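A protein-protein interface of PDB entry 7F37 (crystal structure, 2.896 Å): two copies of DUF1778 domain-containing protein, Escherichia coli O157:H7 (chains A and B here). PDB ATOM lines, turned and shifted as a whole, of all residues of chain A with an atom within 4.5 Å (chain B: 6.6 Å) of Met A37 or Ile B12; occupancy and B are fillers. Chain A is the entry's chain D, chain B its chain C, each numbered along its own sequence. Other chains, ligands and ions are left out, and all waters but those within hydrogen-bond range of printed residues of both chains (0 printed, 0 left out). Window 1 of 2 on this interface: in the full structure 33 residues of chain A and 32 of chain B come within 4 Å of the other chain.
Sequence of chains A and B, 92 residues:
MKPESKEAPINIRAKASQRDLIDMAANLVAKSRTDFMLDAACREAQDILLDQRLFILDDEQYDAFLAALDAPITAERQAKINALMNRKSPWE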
ATOM      1  N   ALA A   8     -13.049  28.356  -6.806  1.00  0.00           N
ATOM      2  CA  ALA A   8     -13.093  26.974  -6.312  1.00  0.00           C
ATOM      3  C   ALA A   8     -12.916  26.973  -4.788  1.00  0.00           C
ATOM      4  O   ALA A   8     -12.133  27.768  -4.260  1.00  0.00           O
ATOM      5  CB  ALA A   8     -12.013  26.114  -6.974  1.00  0.00           C
ATOM      6  N   PRO A   9     -13.587  26.102  -4.041  1.00  0.00           N
ATOM      7  CA  PRO A   9     -13.653  26.285  -2.592  1.00  0.00           C
ATOM      8  C   PRO A   9     -12.573  25.521  -1.847  1.00  0.00           C
ATOM      9  O   PRO A   9     -12.044  24.510  -2.321  1.00  0.00           O
ATOM     10  CB  PRO A   9     -15.036  25.712  -2.260  1.00  0.00           C
ATOM     11  CG  PRO A   9     -15.107  24.515  -3.180  1.00  0.00           C
ATOM     12  CD  PRO A   9     -14.282  24.866  -4.434  1.00  0.00           C
ATOM     13  N   ILE A  10     -12.250  26.025  -0.649  1.00  0.00           N
ATOM     14  CA  ILE A  10     -11.422  25.297   0.314  1.00  0.00           C
ATOM     15  C   ILE A  10     -12.022  25.474   1.705  1.00  0.00           C
ATOM     16  O   ILE A  10     -11.924  26.558   2.291  1.00  0.00           O
ATOM     17  CB  ILE A  10      -9.957  25.743   0.305  1.00  0.00           C
ATOM     18  CG1 ILE A  10      -9.306  25.392  -1.027  1.00  0.00           C
ATOM     19  CG2 ILE A  10      -9.194  25.029   1.401  1.00  0.00           C
ATOM     20  CD1 ILE A  10      -7.901  25.912  -1.166  1.00  0.00           C
ATOM     21  N   ILE A  12     -11.742  24.015   5.573  1.00  0.00           N
ATOM     22  CA  ILE A  12     -10.800  23.300   6.431  1.00  0.00           C
ATOM     23  C   ILE A  12     -11.182  23.508   7.895  1.00  0.00           C
ATOM     24  O   ILE A  12     -11.695  24.562   8.283  1.00  0.00           O
ATOM     25  CB  ILE A  12      -9.336  23.735   6.184  1.00  0.00           C
ATOM     26  CG1 ILE A  12      -9.145  25.231   6.443  1.00  0.00           C
ATOM     27  CG2 ILE A  12      -8.918  23.438   4.771  1.00  0.00           C
ATOM     28  CD1 ILE A  12      -7.693  25.683   6.353  1.00  0.00           C
ATOM     29  N   ILE A  22      -3.942  33.340  13.656  1.00  0.00           N
ATOM     30  CA  ILE A  22      -4.073  33.752  12.257  1.00  0.00           C
ATOM     31  C   ILE A  22      -4.936  35.015  12.133  1.00  0.00           C
ATOM     32  O   ILE A  22      -4.647  35.896  11.316  1.00  0.00           O
ATOM     33  CB  ILE A  22      -4.617  32.596  11.374  1.00  0.00           C
ATOM     34  CG1 ILE A  22      -3.572  31.449  11.109  1.00  0.00           C
ATOM     35  CG2 ILE A  22      -5.282  33.200  10.068  1.00  0.00           C
ATOM     36  CD1 ILE A  22      -3.360  30.363  12.129  1.00  0.00           C
ATOM     37  N   ARG A  33      -9.319  37.011   6.937  1.00  0.00           N
ATOM     38  CA  ARG A  33      -8.753  35.711   7.270  1.00  0.00           C
ATOM     39  C   ARG A  33      -8.530  34.868   6.018  1.00  0.00           C
ATOM     40  O   ARG A  33      -7.444  34.314   5.821  1.00  0.00           O
ATOM     41  CB  ARG A  33      -9.654  34.978   8.260  1.00  0.00           C
ATOM     42  CG  ARG A  33      -9.450  33.475   8.232  1.00  0.00           C
ATOM     43  CD  ARG A  33     -10.136  32.803   9.392  1.00  0.00           C
ATOM     44  NE  ARG A  33     -11.582  32.964   9.334  1.00  0.00           N
ATOM     45  CZ  ARG A  33     -12.321  33.379  10.357  1.00  0.00           C
ATOM     46  NH1 ARG A  33     -11.746  33.674  11.516  1.00  0.00           N
ATOM     47  NH2 ARG A  33     -13.636  33.495  10.224  1.00  0.00           N
ATOM     48  N   THR A  34      -9.551  34.748   5.164  1.00  0.00           N
ATOM     49  CA  THR A  34      -9.371  34.079   3.880  1.00  0.00           C
ATOM     50  C   THR A  34      -8.159  34.649   3.168  1.00  0.00           C
ATOM     51  O   THR A  34      -7.214  33.919   2.852  1.00  0.00           O
ATOM     52  CB  THR A  34     -10.618  34.238   2.994  1.00  0.00           C
ATOM     53  OG1 THR A  34     -10.530  35.450   2.219  1.00  0.00           O
ATOM     54  CG2 THR A  34     -11.842  34.334   3.851  1.00  0.00           C
ATOM     55  N   ASP A  35      -8.167  35.971   2.939  1.00  0.00           N
ATOM     56  CA  ASP A  35      -7.073  36.637   2.244  1.00  0.00           C
ATOM     57  C   ASP A  35      -5.741  36.311   2.896  1.00  0.00           C
ATOM     58  O   ASP A  35      -4.823  35.833   2.229  1.00  0.00           O
ATOM     59  CB  ASP A  35      -7.291  38.147   2.219  1.00  0.00           C
ATOM     60  CG  ASP A  35      -7.982  38.634   0.942  1.00  0.00           C
ATOM     61  OD1 ASP A  35      -7.336  38.761  -0.139  1.00  0.00           O
ATOM     62  OD2 ASP A  35      -9.196  38.911   1.047  1.00  0.00           O
ATOM     63  N   PHE A  36      -5.624  36.542   4.206  1.00  0.00           N
ATOM     64  CA  PHE A  36      -4.422  36.127   4.918  1.00  0.00           C
ATOM     65  C   PHE A  36      -4.044  34.694   4.584  1.00  0.00           C
ATOM     66  O   PHE A  36      -2.983  34.445   4.015  1.00  0.00           O
ATOM     67  CB  PHE A  36      -4.591  36.257   6.432  1.00  0.00           C
ATOM     68  CG  PHE A  36      -3.296  36.056   7.186  1.00  0.00           C
ATOM     69  CD1 PHE A  36      -2.920  34.804   7.642  1.00  0.00           C
ATOM     70  CD2 PHE A  36      -2.428  37.127   7.405  1.00  0.00           C
ATOM     71  CE1 PHE A  36      -1.712  34.627   8.318  1.00  0.00           C
ATOM     72  CE2 PHE A  36      -1.231  36.952   8.082  1.00  0.00           C
ATOM     73  CZ  PHE A  36      -0.871  35.706   8.529  1.00  0.00           C
ATOM     74  N   MET A  37      -4.906  33.735   4.927  1.00  0.00           N
ATOM     75  CA  MET A  37      -4.517  32.334   4.805  1.00  0.00           C
ATOM     76  C   MET A  37      -4.240  31.960   3.373  1.00  0.00           C
ATOM     77  O   MET A  37      -3.545  30.971   3.128  1.00  0.00           O
ATOM     78  CB  MET A  37      -5.594  31.417   5.358  1.00  0.00           C
ATOM     79  CG  MET A  37      -6.003  31.770   6.750  1.00  0.00           C
ATOM     80  SD  MET A  37      -6.672  30.394   7.685  1.00  0.00           S
ATOM     81  CE  MET A  37      -8.066  29.883   6.700  1.00  0.00           C
ATOM     82  N   LEU A  38      -4.764  32.730   2.425  1.00  0.00           N
ATOM     83  CA  LEU A  38      -4.555  32.412   1.020  1.00  0.00           C
ATOM     84  C   LEU A  38      -3.187  32.867   0.556  1.00  0.00           C
ATOM     85  O   LEU A  38      -2.419  32.072   0.003  1.00  0.00           O
ATOM     86  CB  LEU A  38      -5.639  33.053   0.163  1.00  0.00           C
ATOM     87  CG  LEU A  38      -6.638  32.043  -0.378  1.00  0.00           C
ATOM     88  CD1 LEU A  38      -7.335  32.609  -1.618  1.00  0.00           C
ATOM     89  CD2 LEU A  38      -5.936  30.692  -0.641  1.00  0.00           C
ATOM     90  N   ASP A  39      -2.874  34.146   0.770  1.00  0.00           N
ATOM     91  CA  ASP A  39      -1.554  34.657   0.430  1.00  0.00           C
ATOM     92  C   ASP A  39      -0.468  34.038   1.299  1.00  0.00           C
ATOM     93  O   ASP A  39       0.694  34.002   0.892  1.00  0.00           O
ATOM     94  CB  ASP A  39      -1.553  36.189   0.511  1.00  0.00           C
ATOM     95  CG  ASP A  39      -2.676  36.821  -0.362  1.00  0.00           C
ATOM     96  OD1 ASP A  39      -3.870  36.486  -0.167  1.00  0.00           O
ATOM     97  OD2 ASP A  39      -2.371  37.642  -1.264  1.00  0.00           O
ATOM     98  N   ALA A  40      -0.818  33.500   2.456  1.00  0.00           N
ATOM     99  CA  ALA A  40       0.169  32.770   3.235  1.00  0.00           C
ATOM    100  C   ALA A  40       0.485  31.437   2.589  1.00  0.00           C
ATOM    101  O   ALA A  40       1.648  31.023   2.545  1.00  0.00           O
ATOM    102  CB  ALA A  40      -0.335  32.549   4.660  1.00  0.00           C
ATOM    103  N   ALA A  41      -0.543  30.744   2.097  1.00  0.00           N
ATOM    104  CA  ALA A  41      -0.349  29.410   1.550  1.00  0.00           C
ATOM    105  C   ALA A  41       0.319  29.459   0.180  1.00  0.00           C
ATOM    106  O   ALA A  41       1.154  28.602  -0.139  1.00  0.00           O
ATOM    107  CB  ALA A  41      -1.690  28.690   1.473  1.00  0.00           C
ATOM    108  N   ILE B  10     -13.306  27.092   8.528  1.00  0.00           N
ATOM    109  CA  ILE B  10     -12.986  28.357   7.805  1.00  0.00           C
ATOM    110  C   ILE B  10     -13.242  28.069   6.327  1.00  0.00           C
ATOM    111  O   ILE B  10     -12.604  27.156   5.798  1.00  0.00           O
ATOM    112  CB  ILE B  10     -11.526  28.779   8.022  1.00  0.00           C
ATOM    113  CG1 ILE B  10     -11.175  28.845   9.507  1.00  0.00           C
ATOM    114  CG2 ILE B  10     -11.265  30.101   7.328  1.00  0.00           C
ATOM    115  CD1 ILE B  10     -12.111  29.710  10.299  1.00  0.00           C
ATOM    116  N   ASN B  11     -14.126  28.836   5.693  1.00  0.00           N
ATOM    117  CA  ASN B  11     -14.460  28.604   4.264  1.00  0.00           C
ATOM    118  C   ASN B  11     -13.577  29.507   3.414  1.00  0.00           C
ATOM    119  O   ASN B  11     -13.545  30.712   3.682  1.00  0.00           O
ATOM    120  CB  ASN B  11     -15.927  28.919   3.960  1.00  0.00           C
ATOM    121  CG  ASN B  11     -16.333  28.556   2.548  1.00  0.00           C
ATOM    122  OD1 ASN B  11     -15.480  28.412   1.674  1.00  0.00           O
ATOM    123  ND2 ASN B  11     -17.629  28.412   2.318  1.00  0.00           N
ATOM    124  N   ILE B  12     -12.890  28.940   2.428  1.00  0.00           N
ATOM    125  CA  ILE B  12     -12.040  29.812   1.577  1.00  0.00           C
ATOM    126  C   ILE B  12     -12.550  29.782   0.134  1.00  0.00           C
ATOM    127  O   ILE B  12     -12.576  28.701  -0.465  1.00  0.00           O
ATOM    128  CB  ILE B  12     -10.556  29.422   1.691  1.00  0.00           C
ATOM    129  CG1 ILE B  12     -10.116  29.339   3.153  1.00  0.00           C
ATOM    130  CG2 ILE B  12      -9.691  30.384   0.902  1.00  0.00           C
ATOM    131  CD1 ILE B  12      -8.674  29.705   3.376  1.00  0.00           C
ATOM    132  N   ARG B  13     -12.939  30.955  -0.365  1.00  0.00           N
ATOM    133  CA  ARG B  13     -13.361  31.160  -1.752  1.00  0.00           C
ATOM    134  C   ARG B  13     -12.117  31.488  -2.572  1.00  0.00           C
ATOM    135  O   ARG B  13     -11.841  32.633  -2.941  1.00  0.00           O
ATOM    136  CB  ARG B  13     -14.420  32.260  -1.837  1.00  0.00           C
ATOM    137  CG  ARG B  13     -15.464  32.100  -2.959  1.00  0.00           C
ATOM    138  CD  ARG B  13     -15.927  30.639  -3.105  1.00  0.00           C
ATOM    139  NE  ARG B  13     -16.462  30.319  -4.436  1.00  0.00           N
ATOM    140  CZ  ARG B  13     -16.607  29.077  -4.900  1.00  0.00           C
ATOM    141  NH1 ARG B  13     -17.107  28.860  -6.115  1.00  0.00           N
ATOM    142  NH2 ARG B  13     -16.259  28.045  -4.139  1.00  0.00           N
ATOM    143  N   ALA B  14     -11.349  30.441  -2.852  1.00  0.00           N
ATOM    144  CA  ALA B  14     -10.104  30.560  -3.594  1.00  0.00           C
ATOM    145  C   ALA B  14     -10.343  30.585  -5.105  1.00  0.00           C
ATOM    146  O   ALA B  14     -11.288  29.992  -5.622  1.00  0.00           O
ATOM    147  CB  ALA B  14      -9.173  29.401  -3.237  1.00  0.00           C
ATOM    148  N   ARG B  19      -5.780  27.504  -5.900  1.00  0.00           N
ATOM    149  CA  ARG B  19      -6.068  26.189  -5.353  1.00  0.00           C
ATOM    150  C   ARG B  19      -5.210  25.133  -6.033  1.00  0.00           C
ATOM    151  O   ARG B  19      -4.640  24.261  -5.367  1.00  0.00           O
ATOM    152  CB  ARG B  19      -7.552  25.874  -5.509  1.00  0.00           C
ATOM    153  CG  ARG B  19      -8.012  24.766  -4.597  1.00  0.00           C
ATOM    154  CD  ARG B  19      -9.530  24.743  -4.509  1.00  0.00           C
ATOM    155  NE  ARG B  19     -10.131  23.767  -5.415  1.00  0.00           N
ATOM    156  CZ  ARG B  19     -10.036  22.452  -5.254  1.00  0.00           C
ATOM    157  NH1 ARG B  19      -9.356  21.961  -4.226  1.00  0.00           N
ATOM    158  NH2 ARG B  19     -10.616  21.631  -6.119  1.00  0.00           N
ATOM    159  N   ILE B  22      -1.615  25.448  -4.609  1.00  0.00           N
ATOM    160  CA  ILE B  22      -1.376  24.915  -3.271  1.00  0.00           C
ATOM    161  C   ILE B  22      -1.268  23.394  -3.296  1.00  0.00           C
ATOM    162  O   ILE B  22      -0.454  22.808  -2.576  1.00  0.00           O
ATOM    163  CB  ILE B  22      -2.478  25.395  -2.316  1.00  0.00           C
ATOM    164  CG1 ILE B  22      -2.451  26.934  -2.233  1.00  0.00           C
ATOM    165  CG2 ILE B  22      -2.279  24.755  -0.989  1.00  0.00           C
ATOM    166  CD1 ILE B  22      -3.586  27.526  -1.474  1.00  0.00           C
ATOM    167  N   MET B  37      -2.174  24.343   4.171  1.00  0.00           N
ATOM    168  CA  MET B  37      -2.527  25.756   4.164  1.00  0.00           C
ATOM    169  C   MET B  37      -2.656  26.304   5.556  1.00  0.00           C
ATOM    170  O   MET B  37      -2.394  27.488   5.779  1.00  0.00           O
ATOM    171  CB  MET B  37      -3.838  25.977   3.450  1.00  0.00           C
ATOM    172  CG  MET B  37      -3.775  25.705   1.996  1.00  0.00           C
ATOM    173  SD  MET B  37      -5.383  26.098   1.331  1.00  0.00           S
ATOM    174  CE  MET B  37      -5.680  27.690   2.106  1.00  0.00           C
ATOM    175  N   LEU B  38      -3.094  25.463   6.482  1.00  0.00           N
ATOM    176  CA  LEU B  38      -3.261  25.862   7.869  1.00  0.00           C
ATOM    177  C   LEU B  38      -1.941  25.860   8.614  1.00  0.00           C
ATOM    178  O   LEU B  38      -1.741  26.688   9.498  1.00  0.00           O
ATOM    179  CB  LEU B  38      -4.260  24.936   8.549  1.00  0.00           C
ATOM    180  CG  LEU B  38      -4.461  25.153  10.032  1.00  0.00           C
ATOM    181  CD1 LEU B  38      -5.951  25.405  10.338  1.00  0.00           C
ATOM    182  CD2 LEU B  38      -3.907  23.933  10.766  1.00  0.00           C
ATOM    183  N   ALA B  40       0.879  26.567   6.966  1.00  0.00           N
ATOM    184  CA  ALA B  40       1.508  27.739   6.362  1.00  0.00           C
ATOM    185  C   ALA B  40       0.958  29.025   6.953  1.00  0.00           C
ATOM    186  O   ALA B  40       1.722  29.904   7.370  1.00  0.00           O
ATOM    187  CB  ALA B  40       1.290  27.720   4.857  1.00  0.00           C
ATOM    188  N   ALA B  41      -0.373  29.156   6.995  1.00  0.00           N
ATOM    189  CA  ALA B  41      -0.981  30.346   7.577  1.00  0.00           C
ATOM    190  C   ALA B  41      -0.466  30.555   8.990  1.00  0.00           C
ATOM    191  O   ALA B  41       0.114  31.594   9.305  1.00  0.00           O
ATOM    192  CB  ALA B  41      -2.508  30.244   7.553  1.00  0.00           C
ATOM    193  N   CYS B  42      -0.626  29.539   9.832  1.00  0.00           N
ATOM    194  CA  CYS B  42      -0.137  29.583  11.205  1.00  0.00           C
ATOM    195  C   CYS B  42       1.272  30.138  11.268  1.00  0.00           C
ATOM    196  O   CYS B  42       1.560  31.073  12.025  1.00  0.00           O
ATOM    197  CB  CYS B  42      -0.175  28.172  11.789  1.00  0.00           C
ATOM    198  SG  CYS B  42      -0.120  28.044  13.563  1.00  0.00           S
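The backbone carbonyl oxygen of Ala B14 sits at hydrogen-bond distance from the backbone NH of Ala A8.
The backbone nitrogen (N) of Pro A9 lies close to the guanidinium group (NH2) of Arg B13, at 3.3 Å.
N of Ile B10 sits at hydrogen-bond distance from O of Ile A12 (3.0 Å).
The backbone carbonyl oxygen of Ile A10 lies within hydrogen-bond range of the backbone NH of Ile B12.
Among the printed residues, pairs that only touch across the chains: Ala A8 with Ile B12 (3.9 Å), Ala A8 with Arg B13 (3.6 Å), Ala A8 with Arg B19 (3.4 Å), Pro A9 with Ile B12 (3.4 Å), Pro A9 with Arg B19 (3.3 Å), Ile A10 with Ile B10 (3.6 Å), Ile A10 with Asn B11 (3.6 Å), Ile A10 with Arg B19 (3.5 Å), Ile A10 with Met B37 (3.6 Å), Ile A22 with Ala B41 (3.9 Å), Ile A22 with Cys B42 (3.4 Å), Arg A33 with Ile B10 (3.4 Å), Phe A36 with Ala B41 (3.7 Å), Met A37 with Ile B10 (3.3 Å), Met A37 with Ile B12 (3.4 Å), Met A37 with Ala B41 (3.9 Å), Leu A38 with Ile B12 (3.7 Å), Leu A38 with Ala B14 (3.97 Å), Ala A40 with Ala B41 (3.7 Å), Ala A41 with Ile B22 (3.7 Å) and Ala A41 with Met B37 (3.7 Å).
Of the printed residues of chain B, Ile A10 touches Ile B10 (3.6 Å), Asn B11 (3.6 Å), Ile B12 (2.6 Å), Arg B19 (3.5 Å) and Met B37 (3.6 Å).
Printed residues of chain B within 4 Å of Ile A12: Ile B10 (3.0 Å).
Asp A35 touches none of the printed residues of chain B.
Of chain B, only Ile B10, Ile B12 and Ala B41 come within 4 Å of Met A37.
Printed residues of chain B within 4 Å of Ala A41: Ile B22 and Met B37.
Ile B12 touches just these residues of chain A: Ala A8 (3.9 Å), Pro A9 (3.4 Å), Ile A10 (2.6 Å), Met A37 (3.4 Å) and Leu A38 (3.7 Å).
Of the printed residues of chain A, Ile B22 touches Ala A41 (3.7 Å).
Printed residues of chain A within 4 Å of Met B37: Ile A10 (3.6 Å) and Ala A41 (3.7 Å).
The nearest residue of chain B that does not touch Met A37 is Met B37 (4.05 Å).
Of the 14 printed residues of chain A, 11 touch a printed residue of chain B.
Of the 12 printed residues of chain B, 10 touch a printed residue of chain A.
Hydrophobic or aromatic side chains of chain B that line the printed part of chain A: Ile B10, Ile B12, Ala B14, Ile B22, Met B37 and Ala B41.
Among the printed residues, no Asp or Glu carboxylate lies within 4 Å of a Lys or Arg side-chain nitrogen of the other chain.
Ile A10 touches Met B37, and with the chains exchanged Met A37 touches Ile B10.
Ile A22 touches Ala B41, and with the chains exchanged Ala A41 touches Ile B22.
Met A37 touches Ile B12, but with the chains exchanged Ile A12 does not touch Met B37 (4.8 Å).
Met A37 touches Ala B41, and with the chains exchanged Ala A41 touches Met B37.
Of the 25 pairs that touch across the chains among the printed residues, 9 have their exchanged pair printed and touching as well.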
